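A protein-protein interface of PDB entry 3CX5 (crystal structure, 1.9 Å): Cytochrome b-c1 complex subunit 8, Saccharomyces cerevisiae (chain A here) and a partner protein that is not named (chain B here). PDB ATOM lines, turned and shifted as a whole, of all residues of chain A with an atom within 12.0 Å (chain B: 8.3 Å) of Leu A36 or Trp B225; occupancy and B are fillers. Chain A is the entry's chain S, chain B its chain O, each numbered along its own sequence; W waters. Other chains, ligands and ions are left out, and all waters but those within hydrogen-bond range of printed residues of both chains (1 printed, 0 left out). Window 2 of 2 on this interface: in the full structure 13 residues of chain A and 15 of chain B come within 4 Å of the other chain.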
ATOM      1  N   VAL A  28     -14.560 -23.573  22.865  1.00  0.00           N
ATOM      2  CA  VAL A  28     -14.429 -22.280  22.213  1.00  0.00           C
ATOM      3  C   VAL A  28     -15.717 -21.505  22.429  1.00  0.00           C
ATOM      4  O   VAL A  28     -16.813 -22.078  22.460  1.00  0.00           O
ATOM      5  CB  VAL A  28     -14.149 -22.441  20.690  1.00  0.00           C
ATOM      6  CG1 VAL A  28     -14.202 -21.085  19.998  1.00  0.00           C
ATOM      7  CG2 VAL A  28     -12.777 -23.058  20.476  1.00  0.00           C
ATOM      8  N   SER A  29     -15.584 -20.196  22.585  1.00  0.00           N
ATOM      9  CA  SER A  29     -16.739 -19.338  22.810  1.00  0.00           C
ATOM     10  C   SER A  29     -17.751 -19.367  21.673  1.00  0.00           C
ATOM     11  O   SER A  29     -17.379 -19.399  20.501  1.00  0.00           O
ATOM     12  CB  SER A  29     -16.284 -17.893  23.029  1.00  0.00           C
ATOM     13  OG  SER A  29     -17.401 -17.018  23.107  1.00  0.00           O
ATOM     14  N   PRO A  30     -19.054 -19.399  22.016  1.00  0.00           N
ATOM     15  CA  PRO A  30     -20.155 -19.411  21.044  1.00  0.00           C
ATOM     16  C   PRO A  30     -20.038 -18.164  20.159  1.00  0.00           C
ATOM     17  O   PRO A  30     -20.380 -18.191  18.979  1.00  0.00           O
ATOM     18  CB  PRO A  30     -21.391 -19.321  21.937  1.00  0.00           C
ATOM     19  CG  PRO A  30     -20.987 -20.098  23.136  1.00  0.00           C
ATOM     20  CD  PRO A  30     -19.568 -19.607  23.385  1.00  0.00           C
ATOM     21  N   TYR A  31     -19.521 -17.083  20.740  1.00  0.00           N
ATOM     22  CA  TYR A  31     -19.346 -15.819  20.022  1.00  0.00           C
ATOM     23  C   TYR A  31     -18.321 -15.928  18.896  1.00  0.00           C
ATOM     24  O   TYR A  31     -18.351 -15.142  17.944  1.00  0.00           O
ATOM     25  CB  TYR A  31     -18.887 -14.720  20.973  1.00  0.00           C
ATOM     26  CG  TYR A  31     -19.936 -14.227  21.934  1.00  0.00           C
ATOM     27  CD1 TYR A  31     -20.143 -14.858  23.165  1.00  0.00           C
ATOM     28  CD2 TYR A  31     -20.688 -13.092  21.638  1.00  0.00           C
ATOM     29  CE1 TYR A  31     -21.070 -14.353  24.079  1.00  0.00           C
ATOM     30  CE2 TYR A  31     -21.611 -12.591  22.540  1.00  0.00           C
ATOM     31  CZ  TYR A  31     -21.796 -13.219  23.756  1.00  0.00           C
ATOM     32  OH  TYR A  31     -22.684 -12.682  24.654  1.00  0.00           O
ATOM     33  N   ALA A  32     -17.404 -16.886  19.024  1.00  0.00           N
ATOM     34  CA  ALA A  32     -16.358 -17.089  18.031  1.00  0.00           C
ATOM     35  C   ALA A  32     -16.693 -18.159  17.004  1.00  0.00           C
ATOM     36  O   ALA A  32     -15.865 -18.487  16.154  1.00  0.00           O
ATOM     37  CB  ALA A  32     -15.048 -17.418  18.721  1.00  0.00           C
ATOM     38  N   GLN A  33     -17.905 -18.699  17.068  1.00  0.00           N
ATOM     39  CA  GLN A  33     -18.309 -19.748  16.139  1.00  0.00           C
ATOM     40  C   GLN A  33     -19.241 -19.251  15.043  1.00  0.00           C
ATOM     41  O   GLN A  33     -19.900 -18.224  15.196  1.00  0.00           O
ATOM     42  CB  GLN A  33     -18.943 -20.918  16.901  1.00  0.00           C
ATOM     43  CG  GLN A  33     -17.977 -21.614  17.861  1.00  0.00           C
ATOM     44  CD  GLN A  33     -18.603 -22.791  18.594  1.00  0.00           C
ATOM     45  OE1 GLN A  33     -19.279 -23.630  17.993  1.00  0.00           O
ATOM     46  NE2 GLN A  33     -18.370 -22.863  19.899  1.00  0.00           N
ATOM     47  N   LYS A  34     -19.258 -19.978  13.927  1.00  0.00           N
ATOM     48  CA  LYS A  34     -20.101 -19.659  12.773  1.00  0.00           C
ATOM     49  C   LYS A  34     -21.563 -19.628  13.204  1.00  0.00           C
ATOM     50  O   LYS A  34     -22.053 -20.585  13.804  1.00  0.00           O
ATOM     51  CB  LYS A  34     -19.892 -20.702  11.669  1.00  0.00           C
ATOM     52  CG  LYS A  34     -18.480 -20.695  11.093  1.00  0.00           C
ATOM     53  CD  LYS A  34     -18.046 -22.060  10.563  1.00  0.00           C
ATOM     54  CE  LYS A  34     -18.728 -22.425   9.258  1.00  0.00           C
ATOM     55  NZ  LYS A  34     -18.200 -23.716   8.730  1.00  0.00           N
ATOM     56  N   PRO A  35     -22.277 -18.528  12.891  1.00  0.00           N
ATOM     57  CA  PRO A  35     -23.690 -18.280  13.211  1.00  0.00           C
ATOM     58  C   PRO A  35     -24.666 -19.392  12.830  1.00  0.00           C
ATOM     59  O   PRO A  35     -25.523 -19.217  11.962  1.00  0.00           O
ATOM     60  CB  PRO A  35     -23.986 -16.974  12.466  1.00  0.00           C
ATOM     61  CG  PRO A  35     -23.016 -17.000  11.328  1.00  0.00           C
ATOM     62  CD  PRO A  35     -21.763 -17.458  12.019  1.00  0.00           C
ATOM     63  N   LEU A  36     -24.525 -20.525  13.513  1.00  0.00           N
ATOM     64  CA  LEU A  36     -25.360 -21.708  13.328  1.00  0.00           C
ATOM     65  C   LEU A  36     -25.740 -21.979  11.874  1.00  0.00           C
ATOM     66  O   LEU A  36     -26.918 -22.116  11.536  1.00  0.00           O
ATOM     67  CB  LEU A  36     -26.603 -21.592  14.213  1.00  0.00           C
ATOM     68  CG  LEU A  36     -26.262 -21.230  15.663  1.00  0.00           C
ATOM     69  CD1 LEU A  36     -27.524 -20.906  16.432  1.00  0.00           C
ATOM     70  CD2 LEU A  36     -25.479 -22.356  16.326  1.00  0.00           C
ATOM     71  N   GLN A  37     -24.724 -22.027  11.017  1.00  0.00           N
ATOM     72  CA  GLN A  37     -24.918 -22.285   9.594  1.00  0.00           C
ATOM     73  C   GLN A  37     -24.520 -23.717   9.237  1.00  0.00           C
ATOM     74  O   GLN A  37     -24.824 -24.199   8.143  1.00  0.00           O
ATOM     75  CB  GLN A  37     -24.115 -21.285   8.755  1.00  0.00           C
ATOM     76  CG  GLN A  37     -22.620 -21.294   9.031  1.00  0.00           C
ATOM     77  CD  GLN A  37     -21.865 -20.317   8.154  1.00  0.00           C
ATOM     78  OE1 GLN A  37     -21.917 -19.105   8.366  1.00  0.00           O
ATOM     79  NE2 GLN A  37     -21.158 -20.842   7.159  1.00  0.00           N
ATOM     80  N   GLY A  38     -23.835 -24.385  10.164  1.00  0.00           N
ATOM     81  CA  GLY A  38     -23.414 -25.759   9.942  1.00  0.00           C
ATOM     82  C   GLY A  38     -24.511 -26.751  10.288  1.00  0.00           C
ATOM     83  O   GLY A  38     -24.236 -27.828  10.817  1.00  0.00           O
ATOM     84  N   ILE A  39     -25.755 -26.379   9.992  1.00  0.00           N
ATOM     85  CA  ILE A  39     -26.917 -27.221  10.267  1.00  0.00           C
ATOM     86  C   ILE A  39     -27.065 -28.315   9.209  1.00  0.00           C
ATOM     87  O   ILE A  39     -26.745 -29.475   9.468  1.00  0.00           O
ATOM     88  CB  ILE A  39     -28.221 -26.381  10.338  1.00  0.00           C
ATOM     89  CG1 ILE A  39     -28.080 -25.282  11.396  1.00  0.00           C
ATOM     90  CG2 ILE A  39     -29.414 -27.276  10.672  1.00  0.00           C
ATOM     91  CD1 ILE A  39     -29.285 -24.369  11.505  1.00  0.00           C
ATOM     92  N   PHE A  40     -27.536 -27.942   8.020  1.00  0.00           N
ATOM     93  CA  PHE A  40     -27.722 -28.892   6.922  1.00  0.00           C
ATOM     94  C   PHE A  40     -26.391 -29.524   6.522  1.00  0.00           C
ATOM     95  O   PHE A  40     -25.328 -28.931   6.734  1.00  0.00           O
ATOM     96  CB  PHE A  40     -28.351 -28.196   5.710  1.00  0.00           C
ATOM     97  CG  PHE A  40     -29.706 -27.602   5.983  1.00  0.00           C
ATOM     98  CD1 PHE A  40     -29.964 -26.266   5.694  1.00  0.00           C
ATOM     99  CD2 PHE A  40     -30.726 -28.379   6.527  1.00  0.00           C
ATOM    100  CE1 PHE A  40     -31.218 -25.711   5.941  1.00  0.00           C
ATOM    101  CE2 PHE A  40     -31.984 -27.834   6.779  1.00  0.00           C
ATOM    102  CZ  PHE A  40     -32.230 -26.497   6.485  1.00  0.00           C
ATOM    103  N   HIS A  41     -26.459 -30.733   5.964  1.00  0.00           N
ATOM    104  CA  HIS A  41     -25.278 -31.490   5.529  1.00  0.00           C
ATOM    105  C   HIS A  41     -24.489 -32.049   6.719  1.00  0.00           C
ATOM    106  O   HIS A  41     -23.850 -33.098   6.611  1.00  0.00           O
ATOM    107  CB  HIS A  41     -24.377 -30.622   4.631  1.00  0.00           C
ATOM    108  CG  HIS A  41     -23.183 -31.342   4.084  1.00  0.00           C
ATOM    109  ND1 HIS A  41     -23.287 -32.408   3.218  1.00  0.00           N
ATOM    110  CD2 HIS A  41     -21.857 -31.140   4.274  1.00  0.00           C
ATOM    111  CE1 HIS A  41     -22.078 -32.833   2.897  1.00  0.00           C
ATOM    112  NE2 HIS A  41     -21.192 -32.080   3.526  1.00  0.00           N
ATOM    113  N   ASN A  42     -24.548 -31.346   7.847  1.00  0.00           N
ATOM    114  CA  ASN A  42     -23.855 -31.757   9.066  1.00  0.00           C
ATOM    115  C   ASN A  42     -24.845 -32.291  10.103  1.00  0.00           C
ATOM    116  O   ASN A  42     -24.447 -32.749  11.177  1.00  0.00           O
ATOM    117  CB  ASN A  42     -23.074 -30.579   9.657  1.00  0.00           C
ATOM    118  CG  ASN A  42     -22.056 -30.005   8.688  1.00  0.00           C
ATOM    119  OD1 ASN A  42     -22.179 -28.861   8.248  1.00  0.00           O
ATOM    120  ND2 ASN A  42     -21.044 -30.797   8.351  1.00  0.00           N
ATOM    121  N   ALA A  43     -26.133 -32.235   9.769  1.00  0.00           N
ATOM    122  CA  ALA A  43     -27.190 -32.708  10.660  1.00  0.00           C
ATOM    123  C   ALA A  43     -28.335 -33.374   9.901  1.00  0.00           C
ATOM    124  O   ALA A  43     -29.191 -34.014  10.510  1.00  0.00           O
ATOM    125  CB  ALA A  43     -27.719 -31.559  11.513  1.00  0.00           C
ATOM    126  N   VAL A  44     -28.361 -33.210   8.580  1.00  0.00           N
ATOM    127  CA  VAL A  44     -29.406 -33.819   7.760  1.00  0.00           C
ATOM    128  C   VAL A  44     -29.065 -35.283   7.471  1.00  0.00           C
ATOM    129  O   VAL A  44     -29.959 -36.116   7.300  1.00  0.00           O
ATOM    130  CB  VAL A  44     -29.625 -33.046   6.432  1.00  0.00           C
ATOM    131  CG1 VAL A  44     -28.422 -33.199   5.513  1.00  0.00           C
ATOM    132  CG2 VAL A  44     -30.900 -33.521   5.748  1.00  0.00           C
ATOM    133  N   SER B 218     -42.861 -17.824  15.113  1.00  0.00           N
ATOM    134  CA  SER B 218     -41.625 -17.036  15.088  1.00  0.00           C
ATOM    135  C   SER B 218     -40.852 -17.239  16.394  1.00  0.00           C
ATOM    136  O   SER B 218     -39.637 -17.446  16.395  1.00  0.00           O
ATOM    137  CB  SER B 218     -41.953 -15.541  14.925  1.00  0.00           C
ATOM    138  OG  SER B 218     -42.782 -15.298  13.798  1.00  0.00           O
ATOM    139  N   LEU B 219     -41.578 -17.184  17.508  1.00  0.00           N
ATOM    140  CA  LEU B 219     -40.988 -17.372  18.827  1.00  0.00           C
ATOM    141  C   LEU B 219     -40.323 -18.747  18.954  1.00  0.00           C
ATOM    142  O   LEU B 219     -39.230 -18.856  19.499  1.00  0.00           O
ATOM    143  CB  LEU B 219     -42.066 -17.199  19.899  1.00  0.00           C
ATOM    144  CG  LEU B 219     -41.996 -16.055  20.910  1.00  0.00           C
ATOM    145  CD1 LEU B 219     -40.891 -15.061  20.609  1.00  0.00           C
ATOM    146  CD2 LEU B 219     -43.346 -15.384  20.998  1.00  0.00           C
ATOM    147  N   TYR B 220     -40.989 -19.791  18.458  1.00  0.00           N
ATOM    148  CA  TYR B 220     -40.448 -21.148  18.514  1.00  0.00           C
ATOM    149  C   TYR B 220     -39.145 -21.242  17.700  1.00  0.00           C
ATOM    150  O   TYR B 220     -38.136 -21.768  18.184  1.00  0.00           O
ATOM    151  CB  TYR B 220     -41.496 -22.152  18.006  1.00  0.00           C
ATOM    152  CG  TYR B 220     -40.983 -23.554  17.734  1.00  0.00           C
ATOM    153  CD1 TYR B 220     -40.400 -24.327  18.749  1.00  0.00           C
ATOM    154  CD2 TYR B 220     -41.093 -24.114  16.461  1.00  0.00           C
ATOM    155  CE1 TYR B 220     -39.944 -25.621  18.497  1.00  0.00           C
ATOM    156  CE2 TYR B 220     -40.641 -25.399  16.198  1.00  0.00           C
ATOM    157  CZ  TYR B 220     -40.068 -26.148  17.215  1.00  0.00           C
ATOM    158  OH  TYR B 220     -39.630 -27.420  16.941  1.00  0.00           O
ATOM    159  N   LEU B 221     -39.157 -20.695  16.486  1.00  0.00           N
ATOM    160  CA  LEU B 221     -37.965 -20.721  15.633  1.00  0.00           C
ATOM    161  C   LEU B 221     -36.832 -19.908  16.259  1.00  0.00           C
ATOM    162  O   LEU B 221     -35.669 -20.316  16.230  1.00  0.00           O
ATOM    163  CB  LEU B 221     -38.292 -20.181  14.240  1.00  0.00           C
ATOM    164  CG  LEU B 221     -39.261 -21.036  13.421  1.00  0.00           C
ATOM    165  CD1 LEU B 221     -39.806 -20.236  12.227  1.00  0.00           C
ATOM    166  CD2 LEU B 221     -38.564 -22.309  12.966  1.00  0.00           C
ATOM    167  N   LEU B 222     -37.195 -18.765  16.833  1.00  0.00           N
ATOM    168  CA  LEU B 222     -36.251 -17.868  17.487  1.00  0.00           C
ATOM    169  C   LEU B 222     -35.599 -18.560  18.680  1.00  0.00           C
ATOM    170  O   LEU B 222     -34.388 -18.479  18.860  1.00  0.00           O
ATOM    171  CB  LEU B 222     -36.982 -16.610  17.963  1.00  0.00           C
ATOM    172  CG  LEU B 222     -36.766 -15.223  17.345  1.00  0.00           C
ATOM    173  CD1 LEU B 222     -36.085 -15.284  15.998  1.00  0.00           C
ATOM    174  CD2 LEU B 222     -38.101 -14.497  17.266  1.00  0.00           C
ATOM    175  N   SER B 223     -36.401 -19.272  19.473  1.00  0.00           N
ATOM    176  CA  SER B 223     -35.880 -19.958  20.656  1.00  0.00           C
ATOM    177  C   SER B 223     -34.897 -21.072  20.310  1.00  0.00           C
ATOM    178  O   SER B 223     -33.947 -21.322  21.055  1.00  0.00           O
ATOM    179  CB  SER B 223     -37.019 -20.491  21.535  1.00  0.00           C
ATOM    180  OG  SER B 223     -37.684 -21.579  20.929  1.00  0.00           O
ATOM    181  N   ILE B 224     -35.120 -21.740  19.181  1.00  0.00           N
ATOM    182  CA  ILE B 224     -34.229 -22.810  18.742  1.00  0.00           C
ATOM    183  C   ILE B 224     -32.840 -22.219  18.453  1.00  0.00           C
ATOM    184  O   ILE B 224     -31.827 -22.734  18.926  1.00  0.00           O
ATOM    185  CB  ILE B 224     -34.789 -23.513  17.486  1.00  0.00           C
ATOM    186  CG1 ILE B 224     -36.017 -24.348  17.861  1.00  0.00           C
ATOM    187  CG2 ILE B 224     -33.724 -24.383  16.821  1.00  0.00           C
ATOM    188  CD1 ILE B 224     -36.742 -24.915  16.669  1.00  0.00           C
ATOM    189  N   TRP B 225     -32.815 -21.102  17.734  1.00  0.00           N
ATOM    190  CA  TRP B 225     -31.569 -20.424  17.378  1.00  0.00           C
ATOM    191  C   TRP B 225     -30.841 -19.928  18.629  1.00  0.00           C
ATOM    192  O   TRP B 225     -29.621 -20.064  18.745  1.00  0.00           O
ATOM    193  CB  TRP B 225     -31.879 -19.245  16.448  1.00  0.00           C
ATOM    194  CG  TRP B 225     -30.716 -18.773  15.619  1.00  0.00           C
ATOM    195  CD1 TRP B 225     -30.534 -18.978  14.276  1.00  0.00           C
ATOM    196  CD2 TRP B 225     -29.571 -18.028  16.068  1.00  0.00           C
ATOM    197  NE1 TRP B 225     -29.347 -18.411  13.864  1.00  0.00           N
ATOM    198  CE2 TRP B 225     -28.736 -17.824  14.942  1.00  0.00           C
ATOM    199  CE3 TRP B 225     -29.167 -17.516  17.312  1.00  0.00           C
ATOM    200  CZ2 TRP B 225     -27.519 -17.131  15.021  1.00  0.00           C
ATOM    201  CZ3 TRP B 225     -27.959 -16.829  17.390  1.00  0.00           C
ATOM    202  CH2 TRP B 225     -27.149 -16.644  16.248  1.00  0.00           C
ATOM    203  N   VAL B 226     -31.586 -19.319  19.549  1.00  0.00           N
ATOM    204  CA  VAL B 226     -31.002 -18.819  20.787  1.00  0.00           C
ATOM    205  C   VAL B 226     -30.425 -19.984  21.593  1.00  0.00           C
ATOM    206  O   VAL B 226     -29.309 -19.895  22.104  1.00  0.00           O
ATOM    207  CB  VAL B 226     -32.039 -18.027  21.603  1.00  0.00           C
ATOM    208  CG1 VAL B 226     -31.534 -17.745  23.013  1.00  0.00           C
ATOM    209  CG2 VAL B 226     -32.329 -16.705  20.895  1.00  0.00           C
ATOM    210  N   LYS B 227     -31.170 -21.085  21.667  1.00  0.00           N
ATOM    211  CA  LYS B 227     -30.724 -22.270  22.398  1.00  0.00           C
ATOM    212  C   LYS B 227     -29.424 -22.797  21.785  1.00  0.00           C
ATOM    213  O   LYS B 227     -28.463 -23.049  22.497  1.00  0.00           O
ATOM    214  CB  LYS B 227     -31.821 -23.353  22.375  1.00  0.00           C
ATOM    215  CG  LYS B 227     -31.510 -24.652  23.158  1.00  0.00           C
ATOM    216  CD  LYS B 227     -30.709 -25.654  22.336  1.00  0.00           C
ATOM    217  CE  LYS B 227     -30.529 -26.978  23.081  1.00  0.00           C
ATOM    218  NZ  LYS B 227     -29.827 -28.019  22.264  1.00  0.00           N
ATOM    219  N   LYS B 228     -29.387 -22.930  20.459  1.00  0.00           N
ATOM    220  CA  LYS B 228     -28.187 -23.431  19.786  1.00  0.00           C
ATOM    221  C   LYS B 228     -26.972 -22.568  20.081  1.00  0.00           C
ATOM    222  O   LYS B 228     -25.885 -23.097  20.299  1.00  0.00           O
ATOM    223  CB  LYS B 228     -28.403 -23.542  18.273  1.00  0.00           C
ATOM    224  CG  LYS B 228     -29.379 -24.630  17.855  1.00  0.00           C
ATOM    225  CD  LYS B 228     -29.680 -24.537  16.356  1.00  0.00           C
ATOM    226  CE  LYS B 228     -30.441 -25.754  15.851  1.00  0.00           C
ATOM    227  NZ  LYS B 228     -29.623 -26.999  15.954  1.00  0.00           N
ATOM    228  N   PHE B 229     -27.156 -21.246  20.104  1.00  0.00           N
ATOM    229  CA  PHE B 229     -26.057 -20.330  20.403  1.00  0.00           C
ATOM    230  C   PHE B 229     -25.591 -20.535  21.841  1.00  0.00           C
ATOM    231  O   PHE B 229     -24.396 -20.673  22.105  1.00  0.00           O
ATOM    232  CB  PHE B 229     -26.484 -18.864  20.212  1.00  0.00           C
ATOM    233  CG  PHE B 229     -25.392 -17.855  20.535  1.00  0.00           C
ATOM    234  CD1 PHE B 229     -25.374 -17.191  21.761  1.00  0.00           C
ATOM    235  CD2 PHE B 229     -24.386 -17.574  19.608  1.00  0.00           C
ATOM    236  CE1 PHE B 229     -24.363 -16.253  22.065  1.00  0.00           C
ATOM    237  CE2 PHE B 229     -23.371 -16.642  19.896  1.00  0.00           C
ATOM    238  CZ  PHE B 229     -23.361 -15.980  21.130  1.00  0.00           C
ATOM    239  N   LYS B 230     -26.535 -20.573  22.776  1.00  0.00           N
ATOM    240  CA  LYS B 230     -26.169 -20.746  24.180  1.00  0.00           C
ATOM    241  C   LYS B 230     -25.501 -22.090  24.485  1.00  0.00           C
ATOM    242  O   LYS B 230     -24.732 -22.202  25.442  1.00  0.00           O
ATOM    243  CB  LYS B 230     -27.382 -20.516  25.078  1.00  0.00           C
ATOM    244  CG  LYS B 230     -27.847 -19.071  25.061  1.00  0.00           C
ATOM    245  CD  LYS B 230     -29.025 -18.846  25.988  1.00  0.00           C
ATOM    246  CE  LYS B 230     -29.404 -17.380  26.041  1.00  0.00           C
ATOM    247  NZ  LYS B 230     -28.304 -16.571  26.617  1.00  0.00           N
ATOM    248  N   TRP B 231     -25.754 -23.080  23.630  1.00  0.00           N
ATOM    249  CA  TRP B 231     -25.196 -24.418  23.792  1.00  0.00           C
ATOM    250  C   TRP B 231     -23.970 -24.695  22.924  1.00  0.00           C
ATOM    251  O   TRP B 231     -23.374 -25.763  23.039  1.00  0.00           O
ATOM    252  CB  TRP B 231     -26.259 -25.471  23.451  1.00  0.00           C
ATOM    253  CG  TRP B 231     -27.138 -25.857  24.592  1.00  0.00           C
ATOM    254  CD1 TRP B 231     -28.174 -25.135  25.116  1.00  0.00           C
ATOM    255  CD2 TRP B 231     -27.079 -27.083  25.338  1.00  0.00           C
ATOM    256  NE1 TRP B 231     -28.773 -25.844  26.137  1.00  0.00           N
ATOM    257  CE2 TRP B 231     -28.120 -27.038  26.296  1.00  0.00           C
ATOM    258  CE3 TRP B 231     -26.246 -28.210  25.293  1.00  0.00           C
ATOM    259  CZ2 TRP B 231     -28.353 -28.082  27.202  1.00  0.00           C
ATOM    260  CZ3 TRP B 231     -26.476 -29.259  26.200  1.00  0.00           C
ATOM    261  CH2 TRP B 231     -27.525 -29.182  27.139  1.00  0.00           C
ATOM    262  N   ALA B 232     -23.594 -23.747  22.069  1.00  0.00           N
ATOM    263  CA  ALA B 232     -22.477 -23.946  21.142  1.00  0.00           C
ATOM    264  C   ALA B 232     -21.139 -24.322  21.775  1.00  0.00           C
ATOM    265  O   ALA B 232     -20.379 -25.105  21.200  1.00  0.00           O
ATOM    266  CB  ALA B 232     -22.317 -22.731  20.221  1.00  0.00           C
ATOM    267  N   GLY B 233     -20.857 -23.773  22.953  1.00  0.00           N
ATOM    268  CA  GLY B 233     -19.614 -24.079  23.635  1.00  0.00           C
ATOM    269  C   GLY B 233     -19.600 -25.500  24.162  1.00  0.00           C
ATOM    270  O   GLY B 233     -18.559 -26.161  24.147  1.00  0.00           O
ATOM    271  N   LYS B 235     -21.652 -28.080  22.977  1.00  0.00           N
ATOM    272  CA  LYS B 235     -21.807 -28.975  21.832  1.00  0.00           C
ATOM    273  C   LYS B 235     -20.509 -29.320  21.115  1.00  0.00           C
ATOM    274  O   LYS B 235     -20.344 -30.442  20.656  1.00  0.00           O
ATOM    275  CB  LYS B 235     -22.804 -28.396  20.818  1.00  0.00           C
ATOM    276  CG  LYS B 235     -24.266 -28.472  21.243  1.00  0.00           C
ATOM    277  CD  LYS B 235     -24.855 -29.870  21.064  1.00  0.00           C
ATOM    278  CE  LYS B 235     -26.342 -29.860  21.391  1.00  0.00           C
ATOM    279  NZ  LYS B 235     -27.062 -31.053  20.878  1.00  0.00           N
HETATM  280  O   HOH W   1     -16.536 -25.762  22.396  1.00  0.00           O
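O of Ala B232 sits at hydrogen-bond distance from NE2 of Gln A33 (3.3 Å).
The backbone carbonyl oxygen (O) of Val A28 lies within hydrogen-bond range of the side-chain amide nitrogen (NE2) of Gln A33 (3.1 Å). The backbone NH (N) of Tyr A31 sits close to the side-chain hydroxyl (OG) of Ser A29 (3.2 Å).
Gly B233 touches Val A28 (CA to O, 3.6 Å). Phe B229 touches Pro A30. CB of Ala B232 touches CB of Pro A30, at 3.9 Å. Pro A30 touches Gly B233. Phe B229 touches Tyr A31. CD1 of Leu A36 touches O of Trp B225, at 3.2 Å. Leu A36 touches Lys B228 (CD1 to CB, 3.3 Å). Phe B229 touches Leu A36.
Leu A36 touches three residues of chain B. Of chain A, only Leu A36 (3.2 Å) comes within 4 Å of Trp B225. Leu B222 touches none of the printed residues of chain A. No residue of chain A comes within 4 Å of Ile B224. No residue of chain A comes within 4 Å of Val B226. Lys B228 touches one residue of chain A. Of the printed residues of chain A, Phe B229 touches Pro A30 (3.3 Å), Tyr A31 (3.9 Å) and Leu A36 (3.7 Å). Ala B232 touches two residues of chain A. Printed residues of chain B within 4 Å of Tyr A31: Phe B229 (3.9 Å). Printed residues of chain B within 4 Å of Val A28: Gly B233. His A41 touches none of the printed residues of chain B. The nearest printed residue of chain B that does not touch Pro A30 is Lys B230 (4.9 Å).
Of the 17 printed residues of chain B, 5 touch a printed residue of chain A. Hydrophobic or aromatic side chains of chain B within 4 Å of the printed part of chain A: Trp B225, Phe B229 and Ala B232. Of the 17 printed residues of chain A, 5 touch a printed residue of chain B. Hydrophobic or aromatic side chains of chain A within 4 Å of the printed part of chain B: Pro A30, Tyr A31 and Leu A36. Among the printed residues, 9 pairs touch across the chains.
Water W1 bridges O of Gly B233 (2.7 Å) and N of Val A28 (3.0 Å).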
